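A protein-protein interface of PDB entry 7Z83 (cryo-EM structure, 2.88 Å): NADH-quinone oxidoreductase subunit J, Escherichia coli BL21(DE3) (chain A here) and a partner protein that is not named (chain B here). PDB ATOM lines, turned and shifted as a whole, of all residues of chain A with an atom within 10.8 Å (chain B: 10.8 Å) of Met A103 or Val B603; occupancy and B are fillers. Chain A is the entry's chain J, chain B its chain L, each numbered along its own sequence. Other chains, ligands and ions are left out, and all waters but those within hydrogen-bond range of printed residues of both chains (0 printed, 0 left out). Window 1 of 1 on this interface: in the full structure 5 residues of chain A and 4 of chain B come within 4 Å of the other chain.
Met A103 touches just these residues of chain B: Ser B599 and Val B603. Of the printed residues of chain A, Val B603 touches Leu A99, Ile A102 and Met A103. Of chain B, only Ser B599 (3.3 Å), Ile B600 (3.7 Å) and Val B603 (3.7 Å) come within 4 Å of Leu A99. Ser A100 touches none of the printed residues of chain B. Of the printed residues of chain B, Ile A107 touches Leu B606 (3.7 Å). Ser B599 touches just these residues of chain A: Leu A99 (3.3 Å) and Met A103 (3.4 Å). No residue of chain A comes within 4 Å of Gly B601. No residue of chain A comes within 4 Å of Ala B602. No residue of chain A comes within 4 Å of Val B604. Val B605 touches none of the printed residues of chain A. No residue of chain A comes within 4 Å of Ala B607. Of the printed residues of chain A, Ile B600 touches Leu A99 (3.7 Å). Printed residues of chain B within 4 Å of Ile A102: Val B603. Leu B609 touches none of the printed residues of chain A. Pro A96 touches none of the printed residues of chain B. The nearest printed residue of chain A that does not touch Val B603 is Val A106 (5.6 Å). The nearest printed residue of chain B that does not touch Ile A102 is Ala B607 (6.7 Å).
Of the 18 printed residues of chain B, 4 touch a printed residue of chain A. Hydrophobic or aromatic side chains of chain A that line the printed part of chain B: Leu A99, Ile A102, Met A103, Val A106 and Ile A107. Along chain A the printed residues that touch a printed residue of chain B span positions 99 to 107. Among the printed residues, 8 pairs touch across the chains. Among the printed residues, no Asp or Glu carboxylate lies within 4 Å of a Lys or Arg side-chain nitrogen of the other chain.
Leu A99 touches Ser B599. Leu A99 touches Ile B600. CD1 of Leu A99 touches CG2 of Val B603, 3.7 Å away. Ile A102 touches Val B603 (CG2 to CG1, 3.99 Å). Met A103 touches Ser B599 (CE to OG, 3.4 Å). CB of Met A103 touches CG2 of Val B603, at 3.7 Å. Leu B606 touches Val A106. CD2 of Leu B606 touches CG1 of Ile A107 (3.7 Å).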
ATOM      1  N   GLY A  95     -15.421  -5.192 -22.086  1.00  0.00           N
ATOM      2  CA  GLY A  95     -15.603  -6.145 -21.012  1.00  0.00           C
ATOM      3  C   GLY A  95     -16.043  -7.537 -21.443  1.00  0.00           C
ATOM      4  O   GLY A  95     -15.348  -8.529 -21.189  1.00  0.00           O
ATOM      5  N   PRO A  96     -17.229  -7.640 -22.064  1.00  0.00           N
ATOM      6  CA  PRO A  96     -17.694  -8.959 -22.535  1.00  0.00           C
ATOM      7  C   PRO A  96     -16.777  -9.629 -23.546  1.00  0.00           C
ATOM      8  O   PRO A  96     -16.660 -10.860 -23.529  1.00  0.00           O
ATOM      9  CB  PRO A  96     -19.066  -8.640 -23.140  1.00  0.00           C
ATOM     10  CG  PRO A  96     -19.537  -7.467 -22.372  1.00  0.00           C
ATOM     11  CD  PRO A  96     -18.315  -6.642 -22.096  1.00  0.00           C
ATOM     12  N   ALA A  97     -16.118  -8.864 -24.422  1.00  0.00           N
ATOM     13  CA  ALA A  97     -15.184  -9.478 -25.365  1.00  0.00           C
ATOM     14  C   ALA A  97     -13.961 -10.035 -24.649  1.00  0.00           C
ATOM     15  O   ALA A  97     -13.465 -11.107 -25.011  1.00  0.00           O
ATOM     16  CB  ALA A  97     -14.761  -8.476 -26.437  1.00  0.00           C
ATOM     17  N   ILE A  98     -13.467  -9.328 -23.629  1.00  0.00           N
ATOM     18  CA  ILE A  98     -12.349  -9.832 -22.834  1.00  0.00           C
ATOM     19  C   ILE A  98     -12.754 -11.096 -22.083  1.00  0.00           C
ATOM     20  O   ILE A  98     -11.994 -12.071 -22.025  1.00  0.00           O
ATOM     21  CB  ILE A  98     -11.838  -8.727 -21.886  1.00  0.00           C
ATOM     22  CG1 ILE A  98     -10.860  -7.806 -22.622  1.00  0.00           C
ATOM     23  CG2 ILE A  98     -11.196  -9.305 -20.625  1.00  0.00           C
ATOM     24  CD1 ILE A  98      -9.484  -8.405 -22.832  1.00  0.00           C
ATOM     25  N   LEU A  99     -13.969 -11.107 -21.523  1.00  0.00           N
ATOM     26  CA  LEU A  99     -14.465 -12.287 -20.817  1.00  0.00           C
ATOM     27  C   LEU A  99     -14.607 -13.486 -21.752  1.00  0.00           C
ATOM     28  O   LEU A  99     -14.194 -14.607 -21.414  1.00  0.00           O
ATOM     29  CB  LEU A  99     -15.804 -11.957 -20.163  1.00  0.00           C
ATOM     30  CG  LEU A  99     -16.445 -12.988 -19.241  1.00  0.00           C
ATOM     31  CD1 LEU A  99     -15.615 -13.163 -17.983  1.00  0.00           C
ATOM     32  CD2 LEU A  99     -17.851 -12.541 -18.904  1.00  0.00           C
ATOM     33  N   SER A 100     -15.172 -13.263 -22.942  1.00  0.00           N
ATOM     34  CA  SER A 100     -15.335 -14.343 -23.908  1.00  0.00           C
ATOM     35  C   SER A 100     -13.991 -14.821 -24.437  1.00  0.00           C
ATOM     36  O   SER A 100     -13.811 -16.016 -24.690  1.00  0.00           O
ATOM     37  CB  SER A 100     -16.236 -13.889 -25.055  1.00  0.00           C
ATOM     38  OG  SER A 100     -17.600 -14.123 -24.752  1.00  0.00           O
ATOM     39  N   ALA A 101     -13.029 -13.907 -24.598  1.00  0.00           N
ATOM     40  CA  ALA A 101     -11.686 -14.302 -25.004  1.00  0.00           C
ATOM     41  C   ALA A 101     -11.009 -15.150 -23.937  1.00  0.00           C
ATOM     42  O   ALA A 101     -10.338 -16.134 -24.261  1.00  0.00           O
ATOM     43  CB  ALA A 101     -10.847 -13.064 -25.319  1.00  0.00           C
ATOM     44  N   ILE A 102     -11.178 -14.786 -22.661  1.00  0.00           N
ATOM     45  CA  ILE A 102     -10.601 -15.566 -21.567  1.00  0.00           C
ATOM     46  C   ILE A 102     -11.198 -16.969 -21.542  1.00  0.00           C
ATOM     47  O   ILE A 102     -10.473 -17.970 -21.418  1.00  0.00           O
ATOM     48  CB  ILE A 102     -10.811 -14.831 -20.228  1.00  0.00           C
ATOM     49  CG1 ILE A 102      -9.815 -13.677 -20.092  1.00  0.00           C
ATOM     50  CG2 ILE A 102     -10.684 -15.782 -19.045  1.00  0.00           C
ATOM     51  CD1 ILE A 102     -10.195 -12.667 -19.035  1.00  0.00           C
ATOM     52  N   MET A 103     -12.522 -17.063 -21.693  1.00  0.00           N
ATOM     53  CA  MET A 103     -13.170 -18.371 -21.757  1.00  0.00           C
ATOM     54  C   MET A 103     -12.712 -19.158 -22.983  1.00  0.00           C
ATOM     55  O   MET A 103     -12.553 -20.382 -22.918  1.00  0.00           O
ATOM     56  CB  MET A 103     -14.690 -18.195 -21.738  1.00  0.00           C
ATOM     57  CG  MET A 103     -15.493 -19.229 -22.504  1.00  0.00           C
ATOM     58  SD  MET A 103     -17.118 -19.434 -21.763  1.00  0.00           S
ATOM     59  CE  MET A 103     -17.687 -17.743 -21.806  1.00  0.00           C
ATOM     60  N   LEU A 104     -12.462 -18.465 -24.098  1.00  0.00           N
ATOM     61  CA  LEU A 104     -11.970 -19.128 -25.300  1.00  0.00           C
ATOM     62  C   LEU A 104     -10.578 -19.715 -25.089  1.00  0.00           C
ATOM     63  O   LEU A 104     -10.306 -20.837 -25.526  1.00  0.00           O
ATOM     64  CB  LEU A 104     -11.971 -18.148 -26.473  1.00  0.00           C
ATOM     65  CG  LEU A 104     -11.378 -18.631 -27.798  1.00  0.00           C
ATOM     66  CD1 LEU A 104     -12.088 -19.880 -28.294  1.00  0.00           C
ATOM     67  CD2 LEU A 104     -11.443 -17.528 -28.840  1.00  0.00           C
ATOM     68  N   VAL A 105      -9.684 -18.978 -24.421  1.00  0.00           N
ATOM     69  CA  VAL A 105      -8.352 -19.521 -24.138  1.00  0.00           C
ATOM     70  C   VAL A 105      -8.435 -20.688 -23.159  1.00  0.00           C
ATOM     71  O   VAL A 105      -7.686 -21.665 -23.282  1.00  0.00           O
ATOM     72  CB  VAL A 105      -7.385 -18.430 -23.638  1.00  0.00           C
ATOM     73  CG1 VAL A 105      -5.961 -18.948 -23.668  1.00  0.00           C
ATOM     74  CG2 VAL A 105      -7.425 -17.234 -24.550  1.00  0.00           C
ATOM     75  N   VAL A 106      -9.347 -20.617 -22.183  1.00  0.00           N
ATOM     76  CA  VAL A 106      -9.515 -21.736 -21.252  1.00  0.00           C
ATOM     77  C   VAL A 106     -10.001 -22.987 -21.986  1.00  0.00           C
ATOM     78  O   VAL A 106      -9.461 -24.089 -21.799  1.00  0.00           O
ATOM     79  CB  VAL A 106     -10.467 -21.340 -20.107  1.00  0.00           C
ATOM     80  CG1 VAL A 106     -10.862 -22.556 -19.292  1.00  0.00           C
ATOM     81  CG2 VAL A 106      -9.808 -20.308 -19.211  1.00  0.00           C
ATOM     82  N   ILE A 107     -11.000 -22.827 -22.860  1.00  0.00           N
ATOM     83  CA  ILE A 107     -11.535 -23.958 -23.613  1.00  0.00           C
ATOM     84  C   ILE A 107     -10.497 -24.490 -24.599  1.00  0.00           C
ATOM     85  O   ILE A 107     -10.392 -25.702 -24.814  1.00  0.00           O
ATOM     86  CB  ILE A 107     -12.851 -23.551 -24.308  1.00  0.00           C
ATOM     87  CG1 ILE A 107     -13.938 -23.292 -23.267  1.00  0.00           C
ATOM     88  CG2 ILE A 107     -13.353 -24.635 -25.234  1.00  0.00           C
ATOM     89  CD1 ILE A 107     -15.224 -22.748 -23.847  1.00  0.00           C
ATOM     90  N   VAL A 108      -9.688 -23.601 -25.182  1.00  0.00           N
ATOM     91  CA  VAL A 108      -8.643 -24.023 -26.111  1.00  0.00           C
ATOM     92  C   VAL A 108      -7.555 -24.808 -25.383  1.00  0.00           C
ATOM     93  O   VAL A 108      -7.062 -25.825 -25.889  1.00  0.00           O
ATOM     94  CB  VAL A 108      -8.084 -22.793 -26.855  1.00  0.00           C
ATOM     95  CG1 VAL A 108      -6.632 -22.989 -27.280  1.00  0.00           C
ATOM     96  CG2 VAL A 108      -8.949 -22.478 -28.065  1.00  0.00           C
ATOM     97  N   TYR A 109      -7.177 -24.362 -24.180  1.00  0.00           N
ATOM     98  CA  TYR A 109      -6.199 -25.095 -23.379  1.00  0.00           C
ATOM     99  C   TYR A 109      -6.746 -26.462 -22.985  1.00  0.00           C
ATOM    100  O   TYR A 109      -5.999 -27.446 -22.934  1.00  0.00           O
ATOM    101  CB  TYR A 109      -5.803 -24.248 -22.158  1.00  0.00           C
ATOM    102  CG  TYR A 109      -4.817 -24.842 -21.146  1.00  0.00           C
ATOM    103  CD1 TYR A 109      -5.178 -25.867 -20.269  1.00  0.00           C
ATOM    104  CD2 TYR A 109      -3.513 -24.365 -21.080  1.00  0.00           C
ATOM    105  CE1 TYR A 109      -4.275 -26.392 -19.366  1.00  0.00           C
ATOM    106  CE2 TYR A 109      -2.603 -24.886 -20.178  1.00  0.00           C
ATOM    107  CZ  TYR A 109      -2.990 -25.898 -19.326  1.00  0.00           C
ATOM    108  OH  TYR A 109      -2.089 -26.419 -18.426  1.00  0.00           O
ATOM    109  N   ALA A 110      -8.046 -26.538 -22.691  1.00  0.00           N
ATOM    110  CA  ALA A 110      -8.657 -27.834 -22.407  1.00  0.00           C
ATOM    111  C   ALA A 110      -8.674 -28.729 -23.644  1.00  0.00           C
ATOM    112  O   ALA A 110      -8.469 -29.944 -23.540  1.00  0.00           O
ATOM    113  CB  ALA A 110     -10.072 -27.636 -21.871  1.00  0.00           C
ATOM    114  N   ILE A 111      -8.921 -28.144 -24.816  1.00  0.00           N
ATOM    115  CA  ILE A 111      -9.024 -28.915 -26.053  1.00  0.00           C
ATOM    116  C   ILE A 111      -7.662 -29.464 -26.462  1.00  0.00           C
ATOM    117  O   ILE A 111      -7.543 -30.626 -26.869  1.00  0.00           O
ATOM    118  CB  ILE A 111      -9.650 -28.040 -27.158  1.00  0.00           C
ATOM    119  CG1 ILE A 111     -11.172 -28.022 -27.025  1.00  0.00           C
ATOM    120  CG2 ILE A 111      -9.257 -28.516 -28.549  1.00  0.00           C
ATOM    121  CD1 ILE A 111     -11.818 -26.866 -27.741  1.00  0.00           C
ATOM    122  N   LEU A 112      -6.608 -28.656 -26.327  1.00  0.00           N
ATOM    123  CA  LEU A 112      -5.280 -29.043 -26.795  1.00  0.00           C
ATOM    124  C   LEU A 112      -4.658 -30.178 -25.990  1.00  0.00           C
ATOM    125  O   LEU A 112      -3.640 -30.727 -26.422  1.00  0.00           O
ATOM    126  CB  LEU A 112      -4.347 -27.832 -26.774  1.00  0.00           C
ATOM    127  CG  LEU A 112      -4.568 -26.787 -27.869  1.00  0.00           C
ATOM    128  CD1 LEU A 112      -3.801 -25.515 -27.555  1.00  0.00           C
ATOM    129  CD2 LEU A 112      -4.168 -27.339 -29.227  1.00  0.00           C
ATOM    130  N   VAL B 595     -27.147 -12.749 -18.291  1.00  0.00           N
ATOM    131  CA  VAL B 595     -26.332 -13.525 -19.222  1.00  0.00           C
ATOM    132  C   VAL B 595     -24.846 -13.298 -18.956  1.00  0.00           C
ATOM    133  O   VAL B 595     -24.038 -14.236 -19.014  1.00  0.00           O
ATOM    134  CB  VAL B 595     -26.714 -13.181 -20.673  1.00  0.00           C
ATOM    135  CG1 VAL B 595     -25.862 -13.961 -21.646  1.00  0.00           C
ATOM    136  CG2 VAL B 595     -28.183 -13.473 -20.915  1.00  0.00           C
ATOM    137  N   ALA B 596     -24.464 -12.054 -18.650  1.00  0.00           N
ATOM    138  CA  ALA B 596     -23.071 -11.758 -18.324  1.00  0.00           C
ATOM    139  C   ALA B 596     -22.632 -12.476 -17.052  1.00  0.00           C
ATOM    140  O   ALA B 596     -21.504 -12.968 -16.969  1.00  0.00           O
ATOM    141  CB  ALA B 596     -22.874 -10.250 -18.183  1.00  0.00           C
ATOM    142  N   SER B 597     -23.516 -12.555 -16.056  1.00  0.00           N
ATOM    143  CA  SER B 597     -23.199 -13.270 -14.824  1.00  0.00           C
ATOM    144  C   SER B 597     -23.115 -14.772 -15.062  1.00  0.00           C
ATOM    145  O   SER B 597     -22.299 -15.456 -14.436  1.00  0.00           O
ATOM    146  CB  SER B 597     -24.241 -12.957 -13.752  1.00  0.00           C
ATOM    147  OG  SER B 597     -25.439 -13.672 -13.990  1.00  0.00           O
ATOM    148  N   MET B 598     -23.954 -15.299 -15.957  1.00  0.00           N
ATOM    149  CA  MET B 598     -23.855 -16.709 -16.328  1.00  0.00           C
ATOM    150  C   MET B 598     -22.521 -17.011 -17.000  1.00  0.00           C
ATOM    151  O   MET B 598     -21.880 -18.028 -16.704  1.00  0.00           O
ATOM    152  CB  MET B 598     -25.016 -17.088 -17.247  1.00  0.00           C
ATOM    153  CG  MET B 598     -25.320 -18.572 -17.291  1.00  0.00           C
ATOM    154  SD  MET B 598     -27.090 -18.882 -17.402  1.00  0.00           S
ATOM    155  CE  MET B 598     -27.670 -17.994 -15.960  1.00  0.00           C
ATOM    156  N   SER B 599     -22.076 -16.126 -17.896  1.00  0.00           N
ATOM    157  CA  SER B 599     -20.777 -16.316 -18.536  1.00  0.00           C
ATOM    158  C   SER B 599     -19.628 -16.138 -17.546  1.00  0.00           C
ATOM    159  O   SER B 599     -18.613 -16.837 -17.648  1.00  0.00           O
ATOM    160  CB  SER B 599     -20.624 -15.355 -19.713  1.00  0.00           C
ATOM    161  OG  SER B 599     -19.267 -15.246 -20.103  1.00  0.00           O
ATOM    162  N   ILE B 600     -19.778 -15.222 -16.584  1.00  0.00           N
ATOM    163  CA  ILE B 600     -18.783 -15.051 -15.525  1.00  0.00           C
ATOM    164  C   ILE B 600     -18.677 -16.319 -14.686  1.00  0.00           C
ATOM    165  O   ILE B 600     -17.575 -16.775 -14.357  1.00  0.00           O
ATOM    166  CB  ILE B 600     -19.140 -13.822 -14.662  1.00  0.00           C
ATOM    167  CG1 ILE B 600     -18.660 -12.534 -15.329  1.00  0.00           C
ATOM    168  CG2 ILE B 600     -18.551 -13.924 -13.259  1.00  0.00           C
ATOM    169  CD1 ILE B 600     -19.340 -11.289 -14.804  1.00  0.00           C
ATOM    170  N   GLY B 601     -19.821 -16.915 -14.344  1.00  0.00           N
ATOM    171  CA  GLY B 601     -19.809 -18.164 -13.603  1.00  0.00           C
ATOM    172  C   GLY B 601     -19.210 -19.310 -14.393  1.00  0.00           C
ATOM    173  O   GLY B 601     -18.523 -20.166 -13.830  1.00  0.00           O
ATOM    174  N   ALA B 602     -19.456 -19.339 -15.706  1.00  0.00           N
ATOM    175  CA  ALA B 602     -18.824 -20.344 -16.558  1.00  0.00           C
ATOM    176  C   ALA B 602     -17.308 -20.187 -16.569  1.00  0.00           C
ATOM    177  O   ALA B 602     -16.572 -21.178 -16.463  1.00  0.00           O
ATOM    178  CB  ALA B 602     -19.382 -20.257 -17.977  1.00  0.00           C
ATOM    179  N   VAL B 603     -16.829 -18.942 -16.672  1.00  0.00           N
ATOM    180  CA  VAL B 603     -15.392 -18.672 -16.644  1.00  0.00           C
ATOM    181  C   VAL B 603     -14.794 -19.087 -15.306  1.00  0.00           C
ATOM    182  O   VAL B 603     -13.732 -19.719 -15.254  1.00  0.00           O
ATOM    183  CB  VAL B 603     -15.127 -17.184 -16.950  1.00  0.00           C
ATOM    184  CG1 VAL B 603     -13.690 -16.803 -16.622  1.00  0.00           C
ATOM    185  CG2 VAL B 603     -15.428 -16.883 -18.401  1.00  0.00           C
ATOM    186  N   VAL B 604     -15.481 -18.762 -14.207  1.00  0.00           N
ATOM    187  CA  VAL B 604     -14.984 -19.085 -12.870  1.00  0.00           C
ATOM    188  C   VAL B 604     -14.928 -20.596 -12.661  1.00  0.00           C
ATOM    189  O   VAL B 604     -13.931 -21.124 -12.151  1.00  0.00           O
ATOM    190  CB  VAL B 604     -15.854 -18.386 -11.806  1.00  0.00           C
ATOM    191  CG1 VAL B 604     -15.660 -19.016 -10.432  1.00  0.00           C
ATOM    192  CG2 VAL B 604     -15.532 -16.903 -11.755  1.00  0.00           C
ATOM    193  N   VAL B 605     -15.978 -21.315 -13.072  1.00  0.00           N
ATOM    194  CA  VAL B 605     -16.022 -22.767 -12.907  1.00  0.00           C
ATOM    195  C   VAL B 605     -14.936 -23.438 -13.742  1.00  0.00           C
ATOM    196  O   VAL B 605     -14.224 -24.329 -13.257  1.00  0.00           O
ATOM    197  CB  VAL B 605     -17.428 -23.295 -13.258  1.00  0.00           C
ATOM    198  CG1 VAL B 605     -17.401 -24.787 -13.560  1.00  0.00           C
ATOM    199  CG2 VAL B 605     -18.400 -23.001 -12.128  1.00  0.00           C
ATOM    200  N   LEU B 606     -14.772 -23.003 -14.996  1.00  0.00           N
ATOM    201  CA  LEU B 606     -13.756 -23.604 -15.854  1.00  0.00           C
ATOM    202  C   LEU B 606     -12.345 -23.292 -15.363  1.00  0.00           C
ATOM    203  O   LEU B 606     -11.465 -24.156 -15.410  1.00  0.00           O
ATOM    204  CB  LEU B 606     -13.947 -23.136 -17.294  1.00  0.00           C
ATOM    205  CG  LEU B 606     -14.593 -24.166 -18.221  1.00  0.00           C
ATOM    206  CD1 LEU B 606     -16.058 -24.359 -17.874  1.00  0.00           C
ATOM    207  CD2 LEU B 606     -14.441 -23.741 -19.662  1.00  0.00           C
ATOM    208  N   ALA B 607     -12.114 -22.069 -14.873  1.00  0.00           N
ATOM    209  CA  ALA B 607     -10.802 -21.718 -14.339  1.00  0.00           C
ATOM    210  C   ALA B 607     -10.492 -22.494 -13.066  1.00  0.00           C
ATOM    211  O   ALA B 607      -9.348 -22.914 -12.854  1.00  0.00           O
ATOM    212  CB  ALA B 607     -10.727 -20.214 -14.083  1.00  0.00           C
ATOM    213  N   LEU B 608     -11.496 -22.691 -12.205  1.00  0.00           N
ATOM    214  CA  LEU B 608     -11.301 -23.485 -10.998  1.00  0.00           C
ATOM    215  C   LEU B 608     -11.010 -24.941 -11.335  1.00  0.00           C
ATOM    216  O   LEU B 608     -10.175 -25.579 -10.682  1.00  0.00           O
ATOM    217  CB  LEU B 608     -12.531 -23.381 -10.098  1.00  0.00           C
ATOM    218  CG  LEU B 608     -12.596 -22.172  -9.166  1.00  0.00           C
ATOM    219  CD1 LEU B 608     -13.977 -22.053  -8.544  1.00  0.00           C
ATOM    220  CD2 LEU B 608     -11.528 -22.269  -8.090  1.00  0.00           C
ATOM    221  N   LEU B 609     -11.688 -25.485 -12.348  1.00  0.00           N
ATOM    222  CA  LEU B 609     -11.422 -26.863 -12.750  1.00  0.00           C
ATOM    223  C   LEU B 609     -10.053 -27.009 -13.404  1.00  0.00           C
ATOM    224  O   LEU B 609      -9.399 -28.043 -13.237  1.00  0.00           O
ATOM    225  CB  LEU B 609     -12.520 -27.356 -13.687  1.00  0.00           C
ATOM    226  CG  LEU B 609     -13.751 -27.909 -12.969  1.00  0.00           C
ATOM    227  CD1 LEU B 609     -14.928 -27.986 -13.912  1.00  0.00           C
ATOM    228  CD2 LEU B 609     -13.452 -29.273 -12.376  1.00  0.00           C
ATOM    229  N   MET B 610      -9.604 -25.995 -14.148  1.00  0.00           N
ATOM    230  CA  MET B 610      -8.281 -26.061 -14.762  1.00  0.00           C
ATOM    231  C   MET B 610      -7.176 -25.898 -13.725  1.00  0.00           C
ATOM    232  O   MET B 610      -6.110 -26.512 -13.846  1.00  0.00           O
ATOM    233  CB  MET B 610      -8.152 -24.999 -15.852  1.00  0.00           C
ATOM    234  CG  MET B 610      -8.494 -25.488 -17.252  1.00  0.00           C
ATOM    235  SD  MET B 610     -10.085 -26.329 -17.351  1.00  0.00           S
ATOM    236  CE  MET B 610      -9.565 -28.010 -17.661  1.00  0.00           C
ATOM    237  N   VAL B 611      -7.406 -25.065 -12.707  1.00  0.00           N
ATOM    238  CA  VAL B 611      -6.394 -24.846 -11.676  1.00  0.00           C
ATOM    239  C   VAL B 611      -6.249 -26.083 -10.796  1.00  0.00           C
ATOM    240  O   VAL B 611      -5.134 -26.541 -10.518  1.00  0.00           O
ATOM    241  CB  VAL B 611      -6.742 -23.589 -10.855  1.00  0.00           C
ATOM    242  CG1 VAL B 611      -6.105 -23.635  -9.470  1.00  0.00           C
ATOM    243  CG2 VAL B 611      -6.307 -22.336 -11.597  1.00  0.00           C
ATOM    244  N   LEU B 612      -7.371 -26.662 -10.375  1.00  0.00           N
ATOM    245  CA  LEU B 612      -7.360 -27.772  -9.431  1.00  0.00           C
ATOM    246  C   LEU B 612      -7.135 -29.126 -10.089  1.00  0.00           C
ATOM    247  O   LEU B 612      -7.081 -30.136  -9.379  1.00  0.00           O
ATOM    248  CB  LEU B 612      -8.670 -27.796  -8.639  1.00  0.00           C
ATOM    249  CG  LEU B 612      -8.931 -26.574  -7.758  1.00  0.00           C
ATOM    250  CD1 LEU B 612     -10.412 -26.441  -7.460  1.00  0.00           C
ATOM    251  CD2 LEU B 612      -8.130 -26.656  -6.470  1.00  0.00           C
